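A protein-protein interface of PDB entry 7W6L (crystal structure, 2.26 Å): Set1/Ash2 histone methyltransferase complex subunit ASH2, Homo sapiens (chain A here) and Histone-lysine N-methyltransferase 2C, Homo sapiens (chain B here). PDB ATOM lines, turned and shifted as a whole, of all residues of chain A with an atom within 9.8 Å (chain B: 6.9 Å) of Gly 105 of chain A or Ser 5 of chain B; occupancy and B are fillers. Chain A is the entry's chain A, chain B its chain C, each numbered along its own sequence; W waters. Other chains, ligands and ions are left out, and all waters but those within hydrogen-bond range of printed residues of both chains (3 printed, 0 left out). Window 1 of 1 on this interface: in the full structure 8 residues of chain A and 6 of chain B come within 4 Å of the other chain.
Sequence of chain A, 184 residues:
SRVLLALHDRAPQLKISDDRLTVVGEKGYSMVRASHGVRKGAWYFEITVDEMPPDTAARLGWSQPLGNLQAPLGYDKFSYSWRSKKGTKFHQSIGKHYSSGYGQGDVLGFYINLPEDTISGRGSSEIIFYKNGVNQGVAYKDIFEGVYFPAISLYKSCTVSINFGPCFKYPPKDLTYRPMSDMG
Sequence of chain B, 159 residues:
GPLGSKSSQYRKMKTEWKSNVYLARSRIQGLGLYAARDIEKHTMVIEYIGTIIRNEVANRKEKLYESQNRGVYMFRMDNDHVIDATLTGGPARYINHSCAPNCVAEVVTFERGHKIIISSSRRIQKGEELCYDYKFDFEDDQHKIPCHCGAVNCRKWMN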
ATOM      1  N   ILE A  47     -34.269 -10.363  22.139  1.00  0.00           N
ATOM      2  CA  ILE A  47     -33.335 -11.257  22.814  1.00  0.00           C
ATOM      3  C   ILE A  47     -31.996 -11.180  22.103  1.00  0.00           C
ATOM      4  O   ILE A  47     -31.941 -11.213  20.868  1.00  0.00           O
ATOM      5  CB  ILE A  47     -33.839 -12.711  22.867  1.00  0.00           C
ATOM      6  CG1 ILE A  47     -34.973 -12.837  23.888  1.00  0.00           C
ATOM      7  CG2 ILE A  47     -32.700 -13.670  23.235  1.00  0.00           C
ATOM      8  CD1 ILE A  47     -35.845 -14.039  23.667  1.00  0.00           C
ATOM      9  N   THR A  48     -30.925 -11.052  22.884  1.00  0.00           N
ATOM     10  CA  THR A  48     -29.554 -11.111  22.391  1.00  0.00           C
ATOM     11  C   THR A  48     -28.955 -12.452  22.793  1.00  0.00           C
ATOM     12  O   THR A  48     -29.100 -12.881  23.944  1.00  0.00           O
ATOM     13  CB  THR A  48     -28.709  -9.972  22.964  1.00  0.00           C
ATOM     14  OG1 THR A  48     -29.284  -8.710  22.605  1.00  0.00           O
ATOM     15  CG2 THR A  48     -27.277 -10.041  22.437  1.00  0.00           C
ATOM     16  N   VAL A  49     -28.298 -13.117  21.847  1.00  0.00           N
ATOM     17  CA  VAL A  49     -27.616 -14.376  22.118  1.00  0.00           C
ATOM     18  C   VAL A  49     -26.212 -14.019  22.596  1.00  0.00           C
ATOM     19  O   VAL A  49     -25.351 -13.636  21.801  1.00  0.00           O
ATOM     20  CB  VAL A  49     -27.592 -15.284  20.889  1.00  0.00           C
ATOM     21  CG1 VAL A  49     -26.942 -16.616  21.229  1.00  0.00           C
ATOM     22  CG2 VAL A  49     -29.001 -15.485  20.364  1.00  0.00           C
ATOM     23  N   ASP A  50     -25.989 -14.117  23.907  1.00  0.00           N
ATOM     24  CA  ASP A  50     -24.694 -13.738  24.464  1.00  0.00           C
ATOM     25  C   ASP A  50     -23.637 -14.789  24.168  1.00  0.00           C
ATOM     26  O   ASP A  50     -22.513 -14.459  23.773  1.00  0.00           O
ATOM     27  CB  ASP A  50     -24.809 -13.506  25.972  1.00  0.00           C
ATOM     28  CG  ASP A  50     -25.933 -12.550  26.329  1.00  0.00           C
ATOM     29  OD1 ASP A  50     -26.018 -11.473  25.702  1.00  0.00           O
ATOM     30  OD2 ASP A  50     -26.734 -12.874  27.232  1.00  0.00           O
ATOM     31  N   GLU A  51     -23.976 -16.062  24.359  1.00  0.00           N
ATOM     32  CA  GLU A  51     -23.043 -17.153  24.121  1.00  0.00           C
ATOM     33  C   GLU A  51     -23.807 -18.352  23.581  1.00  0.00           C
ATOM     34  O   GLU A  51     -24.852 -18.715  24.131  1.00  0.00           O
ATOM     35  CB  GLU A  51     -22.292 -17.522  25.402  1.00  0.00           C
ATOM     36  N   MET A  52     -23.298 -18.955  22.505  1.00  0.00           N
ATOM     37  CA  MET A  52     -23.859 -20.192  21.955  1.00  0.00           C
ATOM     38  C   MET A  52     -22.732 -21.145  21.596  1.00  0.00           C
ATOM     39  O   MET A  52     -22.302 -21.225  20.440  1.00  0.00           O
ATOM     40  CB  MET A  52     -24.742 -19.923  20.735  1.00  0.00           C
ATOM     41  CG  MET A  52     -25.733 -21.052  20.494  1.00  0.00           C
ATOM     42  SD  MET A  52     -27.140 -20.601  19.475  1.00  0.00           S
ATOM     43  CE  MET A  52     -28.383 -20.323  20.732  1.00  0.00           C
ATOM     44  N   PRO A  53     -22.239 -21.906  22.565  1.00  0.00           N
ATOM     45  CA  PRO A  53     -21.135 -22.827  22.300  1.00  0.00           C
ATOM     46  C   PRO A  53     -21.555 -23.925  21.339  1.00  0.00           C
ATOM     47  O   PRO A  53     -22.751 -24.075  21.038  1.00  0.00           O
ATOM     48  CB  PRO A  53     -20.795 -23.397  23.687  1.00  0.00           C
ATOM     49  CG  PRO A  53     -21.533 -22.578  24.678  1.00  0.00           C
ATOM     50  CD  PRO A  53     -22.641 -21.873  23.980  1.00  0.00           C
ATOM     51  N   GLY A 101     -30.440 -19.447   9.996  1.00  0.00           N
ATOM     52  CA  GLY A 101     -30.165 -19.656  11.399  1.00  0.00           C
ATOM     53  C   GLY A 101     -29.724 -18.382  12.092  1.00  0.00           C
ATOM     54  O   GLY A 101     -29.436 -17.362  11.472  1.00  0.00           O
ATOM     55  N   TYR A 102     -29.689 -18.447  13.421  1.00  0.00           N
ATOM     56  CA  TYR A 102     -29.115 -17.390  14.234  1.00  0.00           C
ATOM     57  C   TYR A 102     -28.221 -18.019  15.290  1.00  0.00           C
ATOM     58  O   TYR A 102     -28.313 -19.215  15.576  1.00  0.00           O
ATOM     59  CB  TYR A 102     -30.200 -16.494  14.871  1.00  0.00           C
ATOM     60  CG  TYR A 102     -31.154 -17.180  15.832  1.00  0.00           C
ATOM     61  CD1 TYR A 102     -30.787 -17.424  17.154  1.00  0.00           C
ATOM     62  CD2 TYR A 102     -32.435 -17.548  15.428  1.00  0.00           C
ATOM     63  CE1 TYR A 102     -31.656 -18.027  18.034  1.00  0.00           C
ATOM     64  CE2 TYR A 102     -33.317 -18.153  16.309  1.00  0.00           C
ATOM     65  CZ  TYR A 102     -32.918 -18.392  17.609  1.00  0.00           C
ATOM     66  OH  TYR A 102     -33.770 -18.999  18.494  1.00  0.00           O
ATOM     67  N   GLY A 103     -27.341 -17.209  15.847  1.00  0.00           N
ATOM     68  CA  GLY A 103     -26.366 -17.692  16.804  1.00  0.00           C
ATOM     69  C   GLY A 103     -25.767 -16.562  17.603  1.00  0.00           C
ATOM     70  O   GLY A 103     -26.377 -15.504  17.772  1.00  0.00           O
ATOM     71  N   GLN A 104     -24.549 -16.795  18.087  1.00  0.00           N
ATOM     72  CA  GLN A 104     -23.935 -15.893  19.052  1.00  0.00           C
ATOM     73  C   GLN A 104     -23.819 -14.480  18.500  1.00  0.00           C
ATOM     74  O   GLN A 104     -23.362 -14.273  17.370  1.00  0.00           O
ATOM     75  CB  GLN A 104     -22.558 -16.418  19.450  1.00  0.00           C
ATOM     76  CG  GLN A 104     -21.918 -15.665  20.607  1.00  0.00           C
ATOM     77  CD  GLN A 104     -20.762 -16.433  21.218  1.00  0.00           C
ATOM     78  OE1 GLN A 104     -20.835 -17.657  21.398  1.00  0.00           O
ATOM     79  NE2 GLN A 104     -19.690 -15.719  21.554  1.00  0.00           N
ATOM     80  N   GLY A 105     -24.230 -13.501  19.311  1.00  0.00           N
ATOM     81  CA  GLY A 105     -24.130 -12.108  18.948  1.00  0.00           C
ATOM     82  C   GLY A 105     -25.270 -11.577  18.108  1.00  0.00           C
ATOM     83  O   GLY A 105     -25.354 -10.355  17.915  1.00  0.00           O
ATOM     84  N   ASP A 106     -26.138 -12.438  17.584  1.00  0.00           N
ATOM     85  CA  ASP A 106     -27.321 -11.950  16.892  1.00  0.00           C
ATOM     86  C   ASP A 106     -28.288 -11.319  17.889  1.00  0.00           C
ATOM     87  O   ASP A 106     -28.337 -11.690  19.065  1.00  0.00           O
ATOM     88  CB  ASP A 106     -28.023 -13.080  16.139  1.00  0.00           C
ATOM     89  CG  ASP A 106     -27.351 -13.413  14.820  1.00  0.00           C
ATOM     90  OD1 ASP A 106     -26.989 -12.474  14.080  1.00  0.00           O
ATOM     91  OD2 ASP A 106     -27.202 -14.620  14.512  1.00  0.00           O
ATOM     92  N   VAL A 107     -29.054 -10.348  17.410  1.00  0.00           N
ATOM     93  CA  VAL A 107     -30.064  -9.670  18.211  1.00  0.00           C
ATOM     94  C   VAL A 107     -31.414  -9.974  17.579  1.00  0.00           C
ATOM     95  O   VAL A 107     -31.674  -9.568  16.440  1.00  0.00           O
ATOM     96  CB  VAL A 107     -29.808  -8.157  18.287  1.00  0.00           C
ATOM     97  CG1 VAL A 107     -30.952  -7.449  19.001  1.00  0.00           C
ATOM     98  CG2 VAL A 107     -28.483  -7.887  18.982  1.00  0.00           C
ATOM     99  N   LEU A 108     -32.267 -10.691  18.307  1.00  0.00           N
ATOM    100  CA  LEU A 108     -33.484 -11.229  17.727  1.00  0.00           C
ATOM    101  C   LEU A 108     -34.671 -10.400  18.211  1.00  0.00           C
ATOM    102  O   LEU A 108     -34.725  -9.997  19.377  1.00  0.00           O
ATOM    103  CB  LEU A 108     -33.685 -12.700  18.111  1.00  0.00           C
ATOM    104  CG  LEU A 108     -32.668 -13.696  17.523  1.00  0.00           C
ATOM    105  CD1 LEU A 108     -32.453 -13.587  15.993  1.00  0.00           C
ATOM    106  CD2 LEU A 108     -31.356 -13.711  18.293  1.00  0.00           C
ATOM    107  N   LYS A 131     -34.316 -10.561  12.728  1.00  0.00           N
ATOM    108  CA  LYS A 131     -32.909 -10.867  12.950  1.00  0.00           C
ATOM    109  C   LYS A 131     -32.102  -9.617  12.629  1.00  0.00           C
ATOM    110  O   LYS A 131     -32.028  -9.208  11.467  1.00  0.00           O
ATOM    111  CB  LYS A 131     -32.466 -12.056  12.094  1.00  0.00           C
ATOM    112  CG  LYS A 131     -31.015 -12.469  12.295  1.00  0.00           C
ATOM    113  CD  LYS A 131     -30.598 -13.456  11.213  1.00  0.00           C
ATOM    114  CE  LYS A 131     -29.239 -14.067  11.503  1.00  0.00           C
ATOM    115  NZ  LYS A 131     -28.694 -14.783  10.315  1.00  0.00           N
ATOM    116  N   ASN A 132     -31.520  -9.006  13.660  1.00  0.00           N
ATOM    117  CA  ASN A 132     -30.712  -7.797  13.509  1.00  0.00           C
ATOM    118  C   ASN A 132     -31.470  -6.717  12.746  1.00  0.00           C
ATOM    119  O   ASN A 132     -30.950  -6.090  11.822  1.00  0.00           O
ATOM    120  CB  ASN A 132     -29.379  -8.114  12.834  1.00  0.00           C
ATOM    121  CG  ASN A 132     -28.586  -9.149  13.596  1.00  0.00           C
ATOM    122  OD1 ASN A 132     -28.416  -9.038  14.810  1.00  0.00           O
ATOM    123  ND2 ASN A 132     -28.103 -10.165  12.894  1.00  0.00           N
ATOM    124  N   GLY A 133     -32.722  -6.508  13.144  1.00  0.00           N
ATOM    125  CA  GLY A 133     -33.540  -5.478  12.545  1.00  0.00           C
ATOM    126  C   GLY A 133     -34.153  -5.826  11.207  1.00  0.00           C
ATOM    127  O   GLY A 133     -34.858  -4.987  10.634  1.00  0.00           O
ATOM    128  N   THR A 159     -26.367 -19.047  26.433  1.00  0.00           N
ATOM    129  CA  THR A 159     -26.714 -17.918  27.288  1.00  0.00           C
ATOM    130  C   THR A 159     -27.357 -16.834  26.439  1.00  0.00           C
ATOM    131  O   THR A 159     -26.767 -16.387  25.450  1.00  0.00           O
ATOM    132  CB  THR A 159     -25.469 -17.381  28.000  1.00  0.00           C
ATOM    133  OG1 THR A 159     -24.937 -18.402  28.853  1.00  0.00           O
ATOM    134  CG2 THR A 159     -25.802 -16.152  28.835  1.00  0.00           C
ATOM    135  N   VAL A 160     -28.571 -16.420  26.814  1.00  0.00           N
ATOM    136  CA  VAL A 160     -29.257 -15.327  26.138  1.00  0.00           C
ATOM    137  C   VAL A 160     -29.733 -14.317  27.172  1.00  0.00           C
ATOM    138  O   VAL A 160     -29.855 -14.614  28.362  1.00  0.00           O
ATOM    139  CB  VAL A 160     -30.442 -15.812  25.278  1.00  0.00           C
ATOM    140  CG1 VAL A 160     -30.004 -16.949  24.367  1.00  0.00           C
ATOM    141  CG2 VAL A 160     -31.615 -16.218  26.155  1.00  0.00           C
ATOM    142  N   SER A 161     -29.993 -13.102  26.696  1.00  0.00           N
ATOM    143  CA  SER A 161     -30.444 -11.995  27.528  1.00  0.00           C
ATOM    144  C   SER A 161     -31.637 -11.338  26.860  1.00  0.00           C
ATOM    145  O   SER A 161     -31.581 -11.008  25.670  1.00  0.00           O
ATOM    146  CB  SER A 161     -29.336 -10.954  27.744  1.00  0.00           C
ATOM    147  OG  SER A 161     -28.261 -11.504  28.478  1.00  0.00           O
ATOM    148  N   LYS A 169     -32.367  -2.338  20.642  1.00  0.00           N
ATOM    149  CA  LYS A 169     -31.207  -2.188  19.770  1.00  0.00           C
ATOM    150  C   LYS A 169     -31.629  -2.010  18.317  1.00  0.00           C
ATOM    151  O   LYS A 169     -31.082  -1.159  17.607  1.00  0.00           O
ATOM    152  CB  LYS A 169     -30.277  -3.390  19.918  1.00  0.00           C
ATOM    153  CG  LYS A 169     -29.692  -3.543  21.321  1.00  0.00           C
ATOM    154  CD  LYS A 169     -28.610  -4.615  21.342  1.00  0.00           C
ATOM    155  CE  LYS A 169     -28.462  -5.254  22.717  1.00  0.00           C
ATOM    156  NZ  LYS A 169     -27.495  -6.389  22.664  1.00  0.00           N
ATOM    157  N   TYR A 170     -32.605  -2.796  17.856  1.00  0.00           N
ATOM    158  CA  TYR A 170     -33.122  -2.707  16.493  1.00  0.00           C
ATOM    159  C   TYR A 170     -34.628  -2.489  16.544  1.00  0.00           C
ATOM    160  O   TYR A 170     -35.406  -3.420  16.293  1.00  0.00           O
ATOM    161  CB  TYR A 170     -32.798  -3.962  15.690  1.00  0.00           C
ATOM    162  CG  TYR A 170     -31.340  -4.121  15.348  1.00  0.00           C
ATOM    163  CD1 TYR A 170     -30.765  -3.390  14.320  1.00  0.00           C
ATOM    164  CD2 TYR A 170     -30.545  -5.022  16.043  1.00  0.00           C
ATOM    165  CE1 TYR A 170     -29.429  -3.544  13.999  1.00  0.00           C
ATOM    166  CE2 TYR A 170     -29.209  -5.185  15.731  1.00  0.00           C
ATOM    167  CZ  TYR A 170     -28.659  -4.447  14.709  1.00  0.00           C
ATOM    168  OH  TYR A 170     -27.331  -4.610  14.401  1.00  0.00           O
ATOM    169  N   PRO B   2     -16.642 -18.092   8.335  1.00  0.00           N
ATOM    170  CA  PRO B   2     -17.980 -17.488   8.301  1.00  0.00           C
ATOM    171  C   PRO B   2     -18.099 -16.288   9.238  1.00  0.00           C
ATOM    172  O   PRO B   2     -17.580 -16.314  10.352  1.00  0.00           O
ATOM    173  CB  PRO B   2     -18.894 -18.632   8.750  1.00  0.00           C
ATOM    174  CG  PRO B   2     -18.017 -19.508   9.578  1.00  0.00           C
ATOM    175  CD  PRO B   2     -16.647 -19.422   8.967  1.00  0.00           C
ATOM    176  N   LEU B   3     -18.791 -15.244   8.785  1.00  0.00           N
ATOM    177  CA  LEU B   3     -18.849 -13.994   9.531  1.00  0.00           C
ATOM    178  C   LEU B   3     -19.814 -14.035  10.710  1.00  0.00           C
ATOM    179  O   LEU B   3     -19.684 -13.211  11.622  1.00  0.00           O
ATOM    180  CB  LEU B   3     -19.234 -12.858   8.585  1.00  0.00           C
ATOM    181  CG  LEU B   3     -18.058 -12.381   7.730  1.00  0.00           C
ATOM    182  CD1 LEU B   3     -18.434 -11.158   6.913  1.00  0.00           C
ATOM    183  CD2 LEU B   3     -16.859 -12.086   8.629  1.00  0.00           C
ATOM    184  N   GLY B   4     -20.762 -14.966  10.722  1.00  0.00           N
ATOM    185  CA  GLY B   4     -21.763 -14.964  11.776  1.00  0.00           C
ATOM    186  C   GLY B   4     -22.469 -13.621  11.843  1.00  0.00           C
ATOM    187  O   GLY B   4     -22.856 -13.041  10.821  1.00  0.00           O
ATOM    188  N   SER B   5     -22.613 -13.105  13.061  1.00  0.00           N
ATOM    189  CA  SER B   5     -23.254 -11.827  13.320  1.00  0.00           C
ATOM    190  C   SER B   5     -22.275 -10.663  13.332  1.00  0.00           C
ATOM    191  O   SER B   5     -22.665  -9.547  13.695  1.00  0.00           O
ATOM    192  CB  SER B   5     -23.994 -11.881  14.658  1.00  0.00           C
ATOM    193  OG  SER B   5     -23.072 -11.977  15.734  1.00  0.00           O
ATOM    194  N   LYS B   6     -21.019 -10.895  12.942  1.00  0.00           N
ATOM    195  CA  LYS B   6     -19.984  -9.875  13.099  1.00  0.00           C
ATOM    196  C   LYS B   6     -20.213  -8.667  12.202  1.00  0.00           C
ATOM    197  O   LYS B   6     -19.869  -7.546  12.586  1.00  0.00           O
ATOM    198  CB  LYS B   6     -18.610 -10.484  12.832  1.00  0.00           C
ATOM    199  CG  LYS B   6     -18.129 -11.343  13.984  1.00  0.00           C
ATOM    200  CD  LYS B   6     -16.745 -11.896  13.754  1.00  0.00           C
ATOM    201  CE  LYS B   6     -16.352 -12.758  14.940  1.00  0.00           C
ATOM    202  NZ  LYS B   6     -16.396 -11.954  16.192  1.00  0.00           N
ATOM    203  N   SER B   7     -20.785  -8.866  11.014  1.00  0.00           N
ATOM    204  CA  SER B   7     -21.077  -7.737  10.137  1.00  0.00           C
ATOM    205  C   SER B   7     -22.100  -6.803  10.774  1.00  0.00           C
ATOM    206  O   SER B   7     -21.895  -5.585  10.828  1.00  0.00           O
ATOM    207  CB  SER B   7     -21.578  -8.244   8.784  1.00  0.00           C
ATOM    208  OG  SER B   7     -20.541  -8.897   8.078  1.00  0.00           O
ATOM    209  N   SER B   8     -23.209  -7.362  11.268  1.00  0.00           N
ATOM    210  CA  SER B   8     -24.236  -6.547  11.914  1.00  0.00           C
ATOM    211  C   SER B   8     -23.692  -5.862  13.162  1.00  0.00           C
ATOM    212  O   SER B   8     -23.917  -4.665  13.375  1.00  0.00           O
ATOM    213  CB  SER B   8     -25.449  -7.409  12.266  1.00  0.00           C
ATOM    214  OG  SER B   8     -26.118  -7.848  11.099  1.00  0.00           O
ATOM    215  N   GLN B   9     -22.985  -6.615  14.008  1.00  0.00           N
ATOM    216  CA  GLN B   9     -22.389  -6.024  15.202  1.00  0.00           C
ATOM    217  C   GLN B   9     -21.456  -4.881  14.845  1.00  0.00           C
ATOM    218  O   GLN B   9     -21.486  -3.824  15.486  1.00  0.00           O
ATOM    219  CB  GLN B   9     -21.616  -7.073  15.990  1.00  0.00           C
ATOM    220  CG  GLN B   9     -22.464  -8.072  16.712  1.00  0.00           C
ATOM    221  CD  GLN B   9     -21.614  -8.977  17.564  1.00  0.00           C
ATOM    222  OE1 GLN B   9     -21.026  -8.546  18.562  1.00  0.00           O
ATOM    223  NE2 GLN B   9     -21.516 -10.235  17.161  1.00  0.00           N
ATOM    224  N   TYR B  10     -20.604  -5.086  13.838  1.00  0.00           N
ATOM    225  CA  TYR B  10     -19.662  -4.050  13.441  1.00  0.00           C
ATOM    226  C   TYR B  10     -20.390  -2.788  13.008  1.00  0.00           C
ATOM    227  O   TYR B  10     -20.099  -1.691  13.497  1.00  0.00           O
ATOM    228  CB  TYR B  10     -18.762  -4.557  12.318  1.00  0.00           C
ATOM    229  CG  TYR B  10     -17.810  -3.509  11.814  1.00  0.00           C
ATOM    230  CD1 TYR B  10     -16.724  -3.113  12.577  1.00  0.00           C
ATOM    231  CD2 TYR B  10     -18.003  -2.900  10.581  1.00  0.00           C
ATOM    232  CE1 TYR B  10     -15.847  -2.146  12.123  1.00  0.00           C
ATOM    233  CE2 TYR B  10     -17.133  -1.931  10.121  1.00  0.00           C
ATOM    234  CZ  TYR B  10     -16.054  -1.560  10.897  1.00  0.00           C
ATOM    235  OH  TYR B  10     -15.178  -0.597  10.444  1.00  0.00           O
ATOM    236  N   HIS B  42     -19.426  -9.150  25.790  1.00  0.00           N
ATOM    237  CA  HIS B  42     -19.367  -9.514  24.368  1.00  0.00           C
ATOM    238  C   HIS B  42     -19.965  -8.430  23.474  1.00  0.00           C
ATOM    239  O   HIS B  42     -20.594  -8.719  22.454  1.00  0.00           O
ATOM    240  CB  HIS B  42     -20.050 -10.857  24.101  1.00  0.00           C
ATOM    241  CG  HIS B  42     -19.396 -12.011  24.790  1.00  0.00           C
ATOM    242  ND1 HIS B  42     -18.103 -12.401  24.522  1.00  0.00           N
ATOM    243  CD2 HIS B  42     -19.857 -12.861  25.740  1.00  0.00           C
ATOM    244  CE1 HIS B  42     -17.793 -13.439  25.277  1.00  0.00           C
ATOM    245  NE2 HIS B  42     -18.840 -13.738  26.026  1.00  0.00           N
ATOM    246  N   MET B  44     -19.197  -5.239  20.994  1.00  0.00           N
ATOM    247  CA  MET B  44     -18.230  -4.468  20.224  1.00  0.00           C
ATOM    248  C   MET B  44     -18.287  -3.017  20.684  1.00  0.00           C
ATOM    249  O   MET B  44     -19.340  -2.377  20.595  1.00  0.00           O
ATOM    250  CB  MET B  44     -18.534  -4.566  18.734  1.00  0.00           C
ATOM    251  CG  MET B  44     -18.011  -5.822  18.090  1.00  0.00           C
ATOM    252  SD  MET B  44     -18.272  -5.798  16.317  1.00  0.00           S
ATOM    253  CE  MET B  44     -17.866  -7.499  15.913  1.00  0.00           C
HETATM  254  O   HOH W   1     -26.259  -3.568  12.048  1.00  0.00           O
HETATM  255  O   HOH W   2     -25.708  -5.948  16.058  1.00  0.00           O
HETATM  256  O   HOH W   3     -26.257 -12.917  11.429  1.00  0.00           O
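The backbone NH of Val 49 of chain A sits at hydrogen-bond distance from the backbone carbonyl oxygen of Asp 106 of chain A (3.1 Å).
The backbone NH of Asp 50 of chain A lies within hydrogen-bond range of the backbone carbonyl oxygen of Thr 159 of chain A (2.9 Å).
The side-chain hydroxyl (OG) of Ser 161 of chain A is in hydrogen-bond range of the side-chain carboxylate (OD2) of Asp 50 of chain A (2.4 Å).
The side-chain carboxylate (OD2) of Asp 106 of chain A is in hydrogen-bond range of the backbone NH (N) of Gly 103 of chain A (2.9 Å).
OD1 of Asp 106 of chain A sits at hydrogen-bond distance from ND2 of Asn 132 of chain A (2.8 Å).
The side-chain amide nitrogen (NE2) of Gln 9 of chain B lies within hydrogen-bond range of the side-chain hydroxyl (OG) of Ser 5 of chain B, 2.7 Å away.
Of the 11 printed residues of chain B, 4 touch a printed residue of chain A.
Printed residues of chain B that touch a printed residue of chain A: Ser 5, Ser 8, Gln 9 and His 42.
Among the printed residues, 7 pairs touch across the chains.
Among the printed residues, no Asp or Glu carboxylate lies within 4 Å of a Lys or Arg side-chain nitrogen of the other chain.
Water W2 lies within hydrogen-bond range of the side-chain hydroxyl (OH) of Tyr 170 of chain A (2.7 Å), the backbone carbonyl oxygen (O) of Ser 8 of chain B (3.5 Å) and the backbone NH (N) of Gln 9 of chain B (3.5 Å).
Water W3 lies within hydrogen-bond range of the side-chain carboxylate of Asp 106 of chain A, the side-chain amino group of Lys 131 of chain A and the backbone carbonyl oxygen of Gly 4 of chain B.
Water W1 bridges the side-chain hydroxyl of Tyr 170 of chain A (2.8 Å) and the backbone carbonyl oxygen of Ser 8 of chain B (2.9 Å).
Gly 105 of chain A touches just these residues of chain B: Ser 5 (3.3 Å) and Gln 9 (3.7 Å).
Ser 5 of chain B touches just these residues of chain A: Gln 104 (2.8 Å), Gly 105 (3.3 Å) and Asp 106 (3.1 Å).
Printed residues of chain B within 4 Å of Asn 132 of chain A: Ser 8 (3.5 Å).
Of the printed residues of chain B, Asp 50 of chain A touches His 42.
The nearest printed residue of chain B that does not touch Asp 106 of chain A is Gln 9 of chain B (5.1 Å).
His 42 of chain B touches Asp 50 of chain A (CD2 to O, 3.7 Å).
Ser 5 of chain B touches Gly 105 of chain A (OG to C, 3.3 Å).
NE2 of Gln 9 of chain B touches CA of Gly 105 of chain A, 3.7 Å away.
Asp 106 of chain A touches Ser 5 of chain B (OD1 to CB, 3.1 Å).
Asn 132 of chain A touches Ser 8 of chain B (ND2 to OG, 3.5 Å).
Ser 8 of chain B touches Tyr 170 of chain A (O to OH, 3.6 Å).
OG of Ser 5 of chain B sits at hydrogen-bond distance from O of Gln 104 of chain A (2.8 Å).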
